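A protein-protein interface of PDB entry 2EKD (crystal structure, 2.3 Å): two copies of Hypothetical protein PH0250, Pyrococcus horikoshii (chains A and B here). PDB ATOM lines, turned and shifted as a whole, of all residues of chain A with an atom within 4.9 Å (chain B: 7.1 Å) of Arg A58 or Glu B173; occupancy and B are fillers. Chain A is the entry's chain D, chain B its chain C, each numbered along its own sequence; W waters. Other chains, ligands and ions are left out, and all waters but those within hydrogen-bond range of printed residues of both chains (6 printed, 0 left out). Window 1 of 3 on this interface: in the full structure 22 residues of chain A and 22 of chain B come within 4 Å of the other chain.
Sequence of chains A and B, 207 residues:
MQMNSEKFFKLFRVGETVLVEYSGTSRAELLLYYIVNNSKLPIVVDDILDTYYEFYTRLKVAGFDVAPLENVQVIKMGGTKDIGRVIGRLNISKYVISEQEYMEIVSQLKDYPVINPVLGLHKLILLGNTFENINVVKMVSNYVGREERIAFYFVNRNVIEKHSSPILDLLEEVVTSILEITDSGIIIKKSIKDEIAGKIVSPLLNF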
ATOM      1  N   TYR A  22      -1.761  -5.037 -24.128  1.00  0.00           N
ATOM      2  CA  TYR A  22      -2.145  -4.949 -22.732  1.00  0.00           C
ATOM      3  C   TYR A  22      -1.087  -5.571 -21.829  1.00  0.00           C
ATOM      4  O   TYR A  22      -0.091  -6.123 -22.308  1.00  0.00           O
ATOM      5  CB  TYR A  22      -3.502  -5.643 -22.519  1.00  0.00           C
ATOM      6  CG  TYR A  22      -3.485  -7.150 -22.688  1.00  0.00           C
ATOM      7  CD1 TYR A  22      -3.203  -7.992 -21.612  1.00  0.00           C
ATOM      8  CD2 TYR A  22      -3.781  -7.738 -23.922  1.00  0.00           C
ATOM      9  CE1 TYR A  22      -3.222  -9.389 -21.756  1.00  0.00           C
ATOM     10  CE2 TYR A  22      -3.801  -9.126 -24.078  1.00  0.00           C
ATOM     11  CZ  TYR A  22      -3.521  -9.945 -22.996  1.00  0.00           C
ATOM     12  OH  TYR A  22      -3.537 -11.318 -23.156  1.00  0.00           O
ATOM     13  N   GLY A  24      -0.589  -7.503 -17.606  1.00  0.00           N
ATOM     14  CA  GLY A  24      -1.297  -8.297 -16.624  1.00  0.00           C
ATOM     15  C   GLY A  24      -2.245  -7.515 -15.729  1.00  0.00           C
ATOM     16  O   GLY A  24      -3.207  -8.088 -15.216  1.00  0.00           O
ATOM     17  N   GLU A  29      -9.561  -8.757 -20.338  1.00  0.00           N
ATOM     18  CA  GLU A  29     -10.768  -9.543 -20.587  1.00  0.00           C
ATOM     19  C   GLU A  29     -12.008  -8.641 -20.633  1.00  0.00           C
ATOM     20  O   GLU A  29     -13.016  -9.000 -21.239  1.00  0.00           O
ATOM     21  CB  GLU A  29     -10.953 -10.632 -19.523  1.00  0.00           C
ATOM     22  CG  GLU A  29     -11.024 -10.106 -18.104  1.00  0.00           C
ATOM     23  CD  GLU A  29      -9.674 -10.101 -17.408  1.00  0.00           C
ATOM     24  OE1 GLU A  29      -8.639  -9.929 -18.090  1.00  0.00           O
ATOM     25  OE2 GLU A  29      -9.653 -10.263 -16.171  1.00  0.00           O
ATOM     26  N   THR A  51      -6.266 -19.765 -24.368  1.00  0.00           N
ATOM     27  CA  THR A  51      -6.262 -18.427 -23.797  1.00  0.00           C
ATOM     28  C   THR A  51      -7.690 -17.908 -23.629  1.00  0.00           C
ATOM     29  O   THR A  51      -7.967 -17.108 -22.734  1.00  0.00           O
ATOM     30  CB  THR A  51      -5.448 -17.472 -24.685  1.00  0.00           C
ATOM     31  OG1 THR A  51      -4.103 -17.963 -24.775  1.00  0.00           O
ATOM     32  CG2 THR A  51      -5.432 -16.056 -24.101  1.00  0.00           C
ATOM     33  N   GLU A  54      -9.051 -18.760 -20.294  1.00  0.00           N
ATOM     34  CA  GLU A  54      -8.508 -17.941 -19.205  1.00  0.00           C
ATOM     35  C   GLU A  54      -9.307 -16.651 -19.067  1.00  0.00           C
ATOM     36  O   GLU A  54      -9.651 -16.246 -17.956  1.00  0.00           O
ATOM     37  CB  GLU A  54      -7.024 -17.641 -19.456  1.00  0.00           C
ATOM     38  CG  GLU A  54      -6.209 -18.901 -19.768  1.00  0.00           C
ATOM     39  CD  GLU A  54      -4.719 -18.648 -19.939  1.00  0.00           C
ATOM     40  OE1 GLU A  54      -4.340 -17.660 -20.606  1.00  0.00           O
ATOM     41  OE2 GLU A  54      -3.922 -19.457 -19.415  1.00  0.00           O
ATOM     42  N   PHE A  55      -9.612 -16.020 -20.199  1.00  0.00           N
ATOM     43  CA  PHE A  55     -10.397 -14.784 -20.224  1.00  0.00           C
ATOM     44  C   PHE A  55     -11.798 -15.074 -19.684  1.00  0.00           C
ATOM     45  O   PHE A  55     -12.317 -14.361 -18.815  1.00  0.00           O
ATOM     46  CB  PHE A  55     -10.519 -14.258 -21.661  1.00  0.00           C
ATOM     47  CG  PHE A  55      -9.381 -13.380 -22.096  1.00  0.00           C
ATOM     48  CD1 PHE A  55      -8.062 -13.834 -22.044  1.00  0.00           C
ATOM     49  CD2 PHE A  55      -9.628 -12.101 -22.591  1.00  0.00           C
ATOM     50  CE1 PHE A  55      -7.012 -13.030 -22.484  1.00  0.00           C
ATOM     51  CE2 PHE A  55      -8.583 -11.286 -23.032  1.00  0.00           C
ATOM     52  CZ  PHE A  55      -7.273 -11.755 -22.978  1.00  0.00           C
ATOM     53  N   TYR A  56     -12.396 -16.135 -20.218  1.00  0.00           N
ATOM     54  CA  TYR A  56     -13.731 -16.574 -19.833  1.00  0.00           C
ATOM     55  C   TYR A  56     -13.806 -16.814 -18.321  1.00  0.00           C
ATOM     56  O   TYR A  56     -14.727 -16.358 -17.648  1.00  0.00           O
ATOM     57  CB  TYR A  56     -14.062 -17.862 -20.597  1.00  0.00           C
ATOM     58  CG  TYR A  56     -15.292 -18.602 -20.123  1.00  0.00           C
ATOM     59  CD1 TYR A  56     -16.567 -18.220 -20.540  1.00  0.00           C
ATOM     60  CD2 TYR A  56     -15.177 -19.692 -19.264  1.00  0.00           C
ATOM     61  CE1 TYR A  56     -17.699 -18.910 -20.114  1.00  0.00           C
ATOM     62  CE2 TYR A  56     -16.300 -20.388 -18.830  1.00  0.00           C
ATOM     63  CZ  TYR A  56     -17.559 -19.993 -19.257  1.00  0.00           C
ATOM     64  OH  TYR A  56     -18.668 -20.677 -18.816  1.00  0.00           O
ATOM     65  N   THR A  57     -12.818 -17.528 -17.802  1.00  0.00           N
ATOM     66  CA  THR A  57     -12.750 -17.855 -16.383  1.00  0.00           C
ATOM     67  C   THR A  57     -12.625 -16.620 -15.485  1.00  0.00           C
ATOM     68  O   THR A  57     -13.250 -16.550 -14.424  1.00  0.00           O
ATOM     69  CB  THR A  57     -11.559 -18.823 -16.116  1.00  0.00           C
ATOM     70  OG1 THR A  57     -11.885 -20.125 -16.623  1.00  0.00           O
ATOM     71  CG2 THR A  57     -11.270 -18.934 -14.645  1.00  0.00           C
ATOM     72  N   ARG A  58     -11.824 -15.643 -15.900  1.00  0.00           N
ATOM     73  CA  ARG A  58     -11.668 -14.444 -15.089  1.00  0.00           C
ATOM     74  C   ARG A  58     -12.943 -13.619 -15.099  1.00  0.00           C
ATOM     75  O   ARG A  58     -13.303 -13.027 -14.088  1.00  0.00           O
ATOM     76  CB  ARG A  58     -10.474 -13.613 -15.564  1.00  0.00           C
ATOM     77  CG  ARG A  58      -9.127 -14.322 -15.352  1.00  0.00           C
ATOM     78  CD  ARG A  58      -7.960 -13.356 -15.417  1.00  0.00           C
ATOM     79  NE  ARG A  58      -7.834 -12.704 -16.716  1.00  0.00           N
ATOM     80  CZ  ARG A  58      -7.322 -13.276 -17.804  1.00  0.00           C
ATOM     81  NH1 ARG A  58      -6.881 -14.530 -17.765  1.00  0.00           N
ATOM     82  NH2 ARG A  58      -7.239 -12.584 -18.933  1.00  0.00           N
ATOM     83  N   LEU A  59     -13.639 -13.595 -16.233  1.00  0.00           N
ATOM     84  CA  LEU A  59     -14.891 -12.849 -16.339  1.00  0.00           C
ATOM     85  C   LEU A  59     -15.997 -13.509 -15.507  1.00  0.00           C
ATOM     86  O   LEU A  59     -16.767 -12.832 -14.829  1.00  0.00           O
ATOM     87  CB  LEU A  59     -15.321 -12.751 -17.805  1.00  0.00           C
ATOM     88  CG  LEU A  59     -14.415 -11.836 -18.623  1.00  0.00           C
ATOM     89  CD1 LEU A  59     -14.588 -12.107 -20.100  1.00  0.00           C
ATOM     90  CD2 LEU A  59     -14.724 -10.379 -18.268  1.00  0.00           C
ATOM     91  N   LYS A  60     -16.061 -14.834 -15.554  1.00  0.00           N
ATOM     92  CA  LYS A  60     -17.066 -15.577 -14.806  1.00  0.00           C
ATOM     93  C   LYS A  60     -16.912 -15.301 -13.311  1.00  0.00           C
ATOM     94  O   LYS A  60     -17.887 -15.019 -12.617  1.00  0.00           O
ATOM     95  CB  LYS A  60     -16.910 -17.072 -15.080  1.00  0.00           C
ATOM     96  CG  LYS A  60     -18.073 -17.932 -14.608  1.00  0.00           C
ATOM     97  CD  LYS A  60     -17.920 -19.355 -15.129  1.00  0.00           C
ATOM     98  CE  LYS A  60     -19.141 -20.202 -14.807  1.00  0.00           C
ATOM     99  NZ  LYS A  60     -19.372 -20.268 -13.342  1.00  0.00           N
ATOM    100  N   VAL A  61     -15.682 -15.381 -12.816  1.00  0.00           N
ATOM    101  CA  VAL A  61     -15.447 -15.126 -11.401  1.00  0.00           C
ATOM    102  C   VAL A  61     -15.809 -13.683 -11.047  1.00  0.00           C
ATOM    103  O   VAL A  61     -16.225 -13.377  -9.937  1.00  0.00           O
ATOM    104  CB  VAL A  61     -13.971 -15.404 -11.056  1.00  0.00           C
ATOM    105  CG1 VAL A  61     -13.703 -15.062  -9.593  1.00  0.00           C
ATOM    106  CG2 VAL A  61     -13.660 -16.876 -11.277  1.00  0.00           C
ATOM    107  N   ALA A  62     -15.621 -12.786 -12.035  1.00  0.00           N
ATOM    108  CA  ALA A  62     -15.936 -11.381 -11.807  1.00  0.00           C
ATOM    109  C   ALA A  62     -17.450 -11.111 -11.829  1.00  0.00           C
ATOM    110  O   ALA A  62     -17.912  -9.990 -11.674  1.00  0.00           O
ATOM    111  CB  ALA A  62     -15.249 -10.542 -12.886  1.00  0.00           C
ATOM    112  N   HIS A 122       1.000 -13.915 -27.989  1.00  0.00           N
ATOM    113  CA  HIS A 122       2.243 -13.772 -27.227  1.00  0.00           C
ATOM    114  C   HIS A 122       2.800 -15.093 -26.718  1.00  0.00           C
ATOM    115  O   HIS A 122       3.994 -15.204 -26.457  1.00  0.00           O
ATOM    116  CB  HIS A 122       2.060 -12.819 -26.046  1.00  0.00           C
ATOM    117  CG  HIS A 122       0.884 -13.149 -25.187  1.00  0.00           C
ATOM    118  ND1 HIS A 122      -0.400 -12.769 -25.509  1.00  0.00           N
ATOM    119  CD2 HIS A 122       0.793 -13.861 -24.038  1.00  0.00           C
ATOM    120  CE1 HIS A 122      -1.235 -13.233 -24.596  1.00  0.00           C
ATOM    121  NE2 HIS A 122      -0.537 -13.898 -23.694  1.00  0.00           N
ATOM    122  N   ASN A 156      -0.153  -9.684 -24.877  1.00  0.00           N
ATOM    123  CA  ASN A 156       0.430  -9.183 -23.650  1.00  0.00           C
ATOM    124  C   ASN A 156       1.742  -8.546 -24.107  1.00  0.00           C
ATOM    125  O   ASN A 156       2.713  -9.237 -24.409  1.00  0.00           O
ATOM    126  CB  ASN A 156       0.697 -10.319 -22.662  1.00  0.00           C
ATOM    127  CG  ASN A 156       1.121  -9.801 -21.298  1.00  0.00           C
ATOM    128  OD1 ASN A 156       1.965  -8.916 -21.207  1.00  0.00           O
ATOM    129  ND2 ASN A 156       0.545 -10.353 -20.236  1.00  0.00           N
ATOM    130  N   LEU B  19      -2.550 -12.992  -6.244  1.00  0.00           N
ATOM    131  CA  LEU B  19      -1.098 -13.014  -6.283  1.00  0.00           C
ATOM    132  C   LEU B  19      -0.595 -12.009  -5.240  1.00  0.00           C
ATOM    133  O   LEU B  19      -0.904 -10.818  -5.310  1.00  0.00           O
ATOM    134  CB  LEU B  19      -0.587 -12.618  -7.675  1.00  0.00           C
ATOM    135  CG  LEU B  19       0.898 -12.879  -7.932  1.00  0.00           C
ATOM    136  CD1 LEU B  19       1.144 -14.380  -7.963  1.00  0.00           C
ATOM    137  CD2 LEU B  19       1.326 -12.250  -9.251  1.00  0.00           C
ATOM    138  N   SER B 141      -3.413 -20.972 -13.755  1.00  0.00           N
ATOM    139  CA  SER B 141      -4.634 -20.583 -14.450  1.00  0.00           C
ATOM    140  C   SER B 141      -5.689 -21.697 -14.480  1.00  0.00           C
ATOM    141  O   SER B 141      -6.883 -21.417 -14.596  1.00  0.00           O
ATOM    142  CB  SER B 141      -4.322 -20.100 -15.874  1.00  0.00           C
ATOM    143  OG  SER B 141      -3.804 -21.128 -16.698  1.00  0.00           O
ATOM    144  N   VAL B 144      -8.002 -21.135 -11.379  1.00  0.00           N
ATOM    145  CA  VAL B 144      -8.686 -19.860 -11.217  1.00  0.00           C
ATOM    146  C   VAL B 144     -10.186 -20.103 -11.335  1.00  0.00           C
ATOM    147  O   VAL B 144     -10.648 -20.735 -12.285  1.00  0.00           O
ATOM    148  CB  VAL B 144      -8.263 -18.837 -12.305  1.00  0.00           C
ATOM    149  CG1 VAL B 144      -9.149 -17.592 -12.234  1.00  0.00           C
ATOM    150  CG2 VAL B 144      -6.816 -18.439 -12.105  1.00  0.00           C
ATOM    151  N   GLY B 145     -10.941 -19.620 -10.352  1.00  0.00           N
ATOM    152  CA  GLY B 145     -12.381 -19.789 -10.389  1.00  0.00           C
ATOM    153  C   GLY B 145     -12.981 -20.937  -9.595  1.00  0.00           C
ATOM    154  O   GLY B 145     -14.188 -20.931  -9.347  1.00  0.00           O
ATOM    155  N   ILE B 167       7.377 -14.128 -17.684  1.00  0.00           N
ATOM    156  CA  ILE B 167       6.633 -15.041 -16.822  1.00  0.00           C
ATOM    157  C   ILE B 167       5.899 -14.315 -15.699  1.00  0.00           C
ATOM    158  O   ILE B 167       4.783 -14.688 -15.345  1.00  0.00           O
ATOM    159  CB  ILE B 167       7.565 -16.117 -16.222  1.00  0.00           C
ATOM    160  CG1 ILE B 167       8.061 -17.035 -17.342  1.00  0.00           C
ATOM    161  CG2 ILE B 167       6.830 -16.923 -15.159  1.00  0.00           C
ATOM    162  CD1 ILE B 167       6.944 -17.748 -18.106  1.00  0.00           C
ATOM    163  N   LEU B 168       6.516 -13.278 -15.136  1.00  0.00           N
ATOM    164  CA  LEU B 168       5.846 -12.528 -14.082  1.00  0.00           C
ATOM    165  C   LEU B 168       4.609 -11.854 -14.669  1.00  0.00           C
ATOM    166  O   LEU B 168       3.563 -11.814 -14.036  1.00  0.00           O
ATOM    167  CB  LEU B 168       6.761 -11.454 -13.480  1.00  0.00           C
ATOM    168  CG  LEU B 168       6.049 -10.539 -12.467  1.00  0.00           C
ATOM    169  CD1 LEU B 168       5.482 -11.377 -11.330  1.00  0.00           C
ATOM    170  CD2 LEU B 168       7.016  -9.496 -11.916  1.00  0.00           C
ATOM    171  N   ASP B 169       4.730 -11.330 -15.882  1.00  0.00           N
ATOM    172  CA  ASP B 169       3.596 -10.654 -16.495  1.00  0.00           C
ATOM    173  C   ASP B 169       2.484 -11.628 -16.877  1.00  0.00           C
ATOM    174  O   ASP B 169       1.320 -11.252 -16.885  1.00  0.00           O
ATOM    175  CB  ASP B 169       4.044  -9.833 -17.708  1.00  0.00           C
ATOM    176  CG  ASP B 169       3.307  -8.499 -17.807  1.00  0.00           C
ATOM    177  OD1 ASP B 169       2.147  -8.483 -18.279  1.00  0.00           O
ATOM    178  OD2 ASP B 169       3.882  -7.464 -17.392  1.00  0.00           O
ATOM    179  N   LEU B 170       2.835 -12.872 -17.190  1.00  0.00           N
ATOM    180  CA  LEU B 170       1.820 -13.869 -17.522  1.00  0.00           C
ATOM    181  C   LEU B 170       1.055 -14.204 -16.246  1.00  0.00           C
ATOM    182  O   LEU B 170      -0.175 -14.267 -16.247  1.00  0.00           O
ATOM    183  CB  LEU B 170       2.456 -15.140 -18.078  1.00  0.00           C
ATOM    184  CG  LEU B 170       2.880 -15.124 -19.545  1.00  0.00           C
ATOM    185  CD1 LEU B 170       3.596 -16.431 -19.855  1.00  0.00           C
ATOM    186  CD2 LEU B 170       1.656 -14.944 -20.456  1.00  0.00           C
ATOM    187  N   LEU B 171       1.798 -14.420 -15.161  1.00  0.00           N
ATOM    188  CA  LEU B 171       1.211 -14.719 -13.857  1.00  0.00           C
ATOM    189  C   LEU B 171       0.214 -13.636 -13.451  1.00  0.00           C
ATOM    190  O   LEU B 171      -0.890 -13.941 -13.010  1.00  0.00           O
ATOM    191  CB  LEU B 171       2.294 -14.789 -12.780  1.00  0.00           C
ATOM    192  CG  LEU B 171       2.833 -16.143 -12.339  1.00  0.00           C
ATOM    193  CD1 LEU B 171       3.818 -15.931 -11.186  1.00  0.00           C
ATOM    194  CD2 LEU B 171       1.681 -17.039 -11.900  1.00  0.00           C
ATOM    195  N   GLU B 172       0.620 -12.374 -13.582  1.00  0.00           N
ATOM    196  CA  GLU B 172      -0.249 -11.263 -13.210  1.00  0.00           C
ATOM    197  C   GLU B 172      -1.500 -11.234 -14.082  1.00  0.00           C
ATOM    198  O   GLU B 172      -2.567 -10.813 -13.634  1.00  0.00           O
ATOM    199  CB  GLU B 172       0.499  -9.920 -13.309  1.00  0.00           C
ATOM    200  CG  GLU B 172       1.704  -9.811 -12.374  1.00  0.00           C
ATOM    201  CD  GLU B 172       2.221  -8.386 -12.223  1.00  0.00           C
ATOM    202  OE1 GLU B 172       2.136  -7.604 -13.195  1.00  0.00           O
ATOM    203  OE2 GLU B 172       2.728  -8.044 -11.136  1.00  0.00           O
ATOM    204  N   GLU B 173      -1.371 -11.693 -15.321  1.00  0.00           N
ATOM    205  CA  GLU B 173      -2.503 -11.715 -16.240  1.00  0.00           C
ATOM    206  C   GLU B 173      -3.559 -12.757 -15.865  1.00  0.00           C
ATOM    207  O   GLU B 173      -4.762 -12.472 -15.897  1.00  0.00           O
ATOM    208  CB  GLU B 173      -2.026 -11.994 -17.668  1.00  0.00           C
ATOM    209  CG  GLU B 173      -3.156 -12.134 -18.692  1.00  0.00           C
ATOM    210  CD  GLU B 173      -2.651 -12.459 -20.104  1.00  0.00           C
ATOM    211  OE1 GLU B 173      -1.472 -12.156 -20.412  1.00  0.00           O
ATOM    212  OE2 GLU B 173      -3.443 -13.000 -20.914  1.00  0.00           O
ATOM    213  N   VAL B 174      -3.111 -13.959 -15.509  1.00  0.00           N
ATOM    214  CA  VAL B 174      -4.038 -15.036 -15.183  1.00  0.00           C
ATOM    215  C   VAL B 174      -4.740 -14.984 -13.825  1.00  0.00           C
ATOM    216  O   VAL B 174      -5.782 -15.621 -13.657  1.00  0.00           O
ATOM    217  CB  VAL B 174      -3.357 -16.417 -15.319  1.00  0.00           C
ATOM    218  CG1 VAL B 174      -2.868 -16.620 -16.758  1.00  0.00           C
ATOM    219  CG2 VAL B 174      -2.207 -16.537 -14.317  1.00  0.00           C
ATOM    220  N   VAL B 175      -4.188 -14.255 -12.852  1.00  0.00           N
ATOM    221  CA  VAL B 175      -4.848 -14.178 -11.542  1.00  0.00           C
ATOM    222  C   VAL B 175      -5.928 -13.100 -11.581  1.00  0.00           C
ATOM    223  O   VAL B 175      -5.942 -12.266 -12.481  1.00  0.00           O
ATOM    224  CB  VAL B 175      -3.837 -13.898 -10.384  1.00  0.00           C
ATOM    225  CG1 VAL B 175      -2.757 -14.989 -10.373  1.00  0.00           C
ATOM    226  CG2 VAL B 175      -3.209 -12.502 -10.523  1.00  0.00           C
ATOM    227  N   THR B 176      -6.838 -13.123 -10.612  1.00  0.00           N
ATOM    228  CA  THR B 176      -7.937 -12.155 -10.570  1.00  0.00           C
ATOM    229  C   THR B 176      -7.627 -10.922  -9.723  1.00  0.00           C
ATOM    230  O   THR B 176      -8.166  -9.835  -9.951  1.00  0.00           O
ATOM    231  CB  THR B 176      -9.232 -12.827 -10.046  1.00  0.00           C
ATOM    232  OG1 THR B 176      -8.932 -13.588  -8.871  1.00  0.00           O
ATOM    233  CG2 THR B 176      -9.823 -13.772 -11.107  1.00  0.00           C
ATOM    234  N   ILE B 178      -4.314  -8.826  -7.424  1.00  0.00           N
ATOM    235  CA  ILE B 178      -2.889  -8.716  -7.183  1.00  0.00           C
ATOM    236  C   ILE B 178      -2.626  -7.741  -6.055  1.00  0.00           C
ATOM    237  O   ILE B 178      -3.077  -6.597  -6.088  1.00  0.00           O
ATOM    238  CB  ILE B 178      -2.128  -8.208  -8.421  1.00  0.00           C
ATOM    239  CG1 ILE B 178      -2.378  -9.132  -9.613  1.00  0.00           C
ATOM    240  CG2 ILE B 178      -0.629  -8.138  -8.104  1.00  0.00           C
ATOM    241  CD1 ILE B 178      -1.793  -8.609 -10.911  1.00  0.00           C
ATOM    242  N   LYS B 190      -4.391  -4.982  -8.736  1.00  0.00           N
ATOM    243  CA  LYS B 190      -5.464  -5.463  -9.598  1.00  0.00           C
ATOM    244  C   LYS B 190      -6.579  -6.052  -8.740  1.00  0.00           C
ATOM    245  O   LYS B 190      -6.325  -6.636  -7.692  1.00  0.00           O
ATOM    246  CB  LYS B 190      -4.943  -6.519 -10.586  1.00  0.00           C
ATOM    247  CG  LYS B 190      -6.000  -6.969 -11.586  1.00  0.00           C
ATOM    248  CD  LYS B 190      -5.428  -7.763 -12.757  1.00  0.00           C
ATOM    249  CE  LYS B 190      -5.495  -9.252 -12.534  1.00  0.00           C
ATOM    250  NZ  LYS B 190      -5.181  -9.993 -13.798  1.00  0.00           N
ATOM    251  N   ILE B 192     -11.072  -7.502  -8.891  1.00  0.00           N
ATOM    252  CA  ILE B 192     -12.343  -7.654  -9.605  1.00  0.00           C
ATOM    253  C   ILE B 192     -13.192  -6.402  -9.427  1.00  0.00           C
ATOM    254  O   ILE B 192     -13.987  -6.010 -10.276  1.00  0.00           O
ATOM    255  CB  ILE B 192     -13.085  -8.860  -9.027  1.00  0.00           C
ATOM    256  CG1 ILE B 192     -12.466 -10.158  -9.542  1.00  0.00           C
ATOM    257  CG2 ILE B 192     -14.550  -8.828  -9.494  1.00  0.00           C
ATOM    258  CD1 ILE B 192     -13.149 -11.401  -8.977  1.00  0.00           C
HETATM  259  O   HOH W   1      -6.977 -16.863 -16.002  1.00  0.00           O
HETATM  260  O   HOH W   2      -4.997 -14.924 -20.201  1.00  0.00           O
HETATM  261  O   HOH W   3      -5.963 -10.047 -16.781  1.00  0.00           O
HETATM  262  O   HOH W   4       1.419  -6.570 -15.344  1.00  0.00           O
HETATM  263  O   HOH W   5      -8.057  -9.633 -14.437  1.00  0.00           O
HETATM  264  O   HOH W   6      -1.969 -15.200 -22.057  1.00  0.00           O
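Gly A24 touches Glu B173 (CA to N, 3.6 Å).
Glu B173 touches Phe A55.
Thr A57 touches Val B144 (CG2 to O, 3.0 Å).
Arg A58 touches Val B174.
Arg A58 touches Val B175 (CD to O, 3.7 Å).
CA of Gly B145 touches CG2 of Val A61, 3.3 Å away.
Val A61 touches Ile B192 (CG1 to CD1, 3.8 Å).
Ala A62 touches Ile B192.
CD2 of Leu B170 touches CD2 of His A122 (3.8 Å).
OE1 of Glu B173 touches NE2 of His A122 (3.8 Å).
The side-chain amino group (NZ) of Lys B190 sits at hydrogen-bond distance from the backbone carbonyl oxygen (O) of Val B175, 2.7 Å away.
OE2 of Glu A29 is in salt-bridge range of NE of Arg A58 (3.1 Å).
The backbone NH (N) of Ile B178 is in hydrogen-bond range of the backbone carbonyl oxygen (O) of Lys B190, at 3.0 Å.
The side-chain amino group (NZ) of Lys B190 is in hydrogen-bond range of the backbone carbonyl oxygen (O) of Glu B173, 3.3 Å away.
The backbone NH of Asn A156 is in hydrogen-bond range of a ring nitrogen (ND1) of His A122 (3.2 Å).
O of Glu B172 lies within hydrogen-bond range of NZ of Lys B190, at 2.7 Å.
No position is printed for both chains.
The backbone carbonyl oxygen (O) of Glu B173 lies within hydrogen-bond range of the guanidinium group (NE) of Arg A58, at 3.2 Å.
OE1 of Glu B173 lies within hydrogen-bond range of ND2 of Asn A156, 2.7 Å away.
The backbone carbonyl oxygen (O) of Gly A24 lies within hydrogen-bond range of the side-chain amino group (NZ) of Lys B190 (3.1 Å).
The backbone carbonyl oxygen (O) of Gly A24 sits close to the backbone carbonyl oxygen (O) of Glu B172 (3.2 Å).
OD1 of Asp B169 lies within hydrogen-bond range of N of Gly A24, 3.0 Å away.
OH of Tyr A22 is in hydrogen-bond range of OE2 of Glu B173 (2.8 Å).
The side-chain amide oxygen (OD1) of Asn A156 lies close to the side-chain carboxylate (OD1) of Asp B169 (3.0 Å).
The side-chain carboxylate of Glu A54 lies within hydrogen-bond range of the side-chain hydroxyl of Ser B141.
Water W5 lies within hydrogen-bond range of OE2 of Glu A29 (2.4 Å) and NZ of Lys B190 (3.0 Å).
Water W4 lies within hydrogen-bond range of OE1 of Glu B172 (2.5 Å), N of Gly A24 (3.2 Å) and OD2 of Asp B169 (3.3 Å).
Water W6 bridges NE2 of His A122 (2.5 Å) and OE2 of Glu B173 (2.9 Å).
Water W2 lies within hydrogen-bond range of the side-chain carboxylate (OE2) of Glu B173, the side-chain carboxylate (OE1) of Glu A54 and the guanidinium group (NH1) of Arg A58.
Water W3 lies within hydrogen-bond range of the backbone carbonyl oxygen (O) of Glu B173 (2.8 Å), the side-chain carboxylate (OE1) of Glu A29 (3.0 Å), the side-chain amino group (NZ) of Lys B190 (3.1 Å) and the guanidinium group (NE) of Arg A58 (3.3 Å).
Water W1 lies within hydrogen-bond range of the backbone carbonyl oxygen of Val B174, the guanidinium group of Arg A58 and the backbone carbonyl oxygen of Glu A54.
Of the printed residues of chain B, Tyr A22 touches Glu B173 (2.8 Å).
Glu A29 touches none of the printed residues of chain B.
Of chain B, only Glu B173 (3.2 Å), Val B174 (3.6 Å) and Val B175 (3.7 Å) come within 4 Å of Arg A58.
Of the printed residues of chain B, His A122 touches Leu B170 (3.8 Å) and Glu B173 (3.8 Å).
Glu B173 touches just these residues of chain A: Tyr A22 (2.8 Å), Gly A24 (3.6 Å), Phe A55 (3.9 Å), Arg A58 (3.2 Å), His A122 (3.8 Å) and Asn A156 (2.7 Å).
The nearest residue of chain A that does not touch Glu B173 is Glu A54 (4.8 Å).
Along chain B the printed residues that touch a printed residue of chain A span positions 141 to 192.
Among the printed residues, no Asp or Glu carboxylate lies within 4 Å of a Lys or Arg side-chain nitrogen of the other chain.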
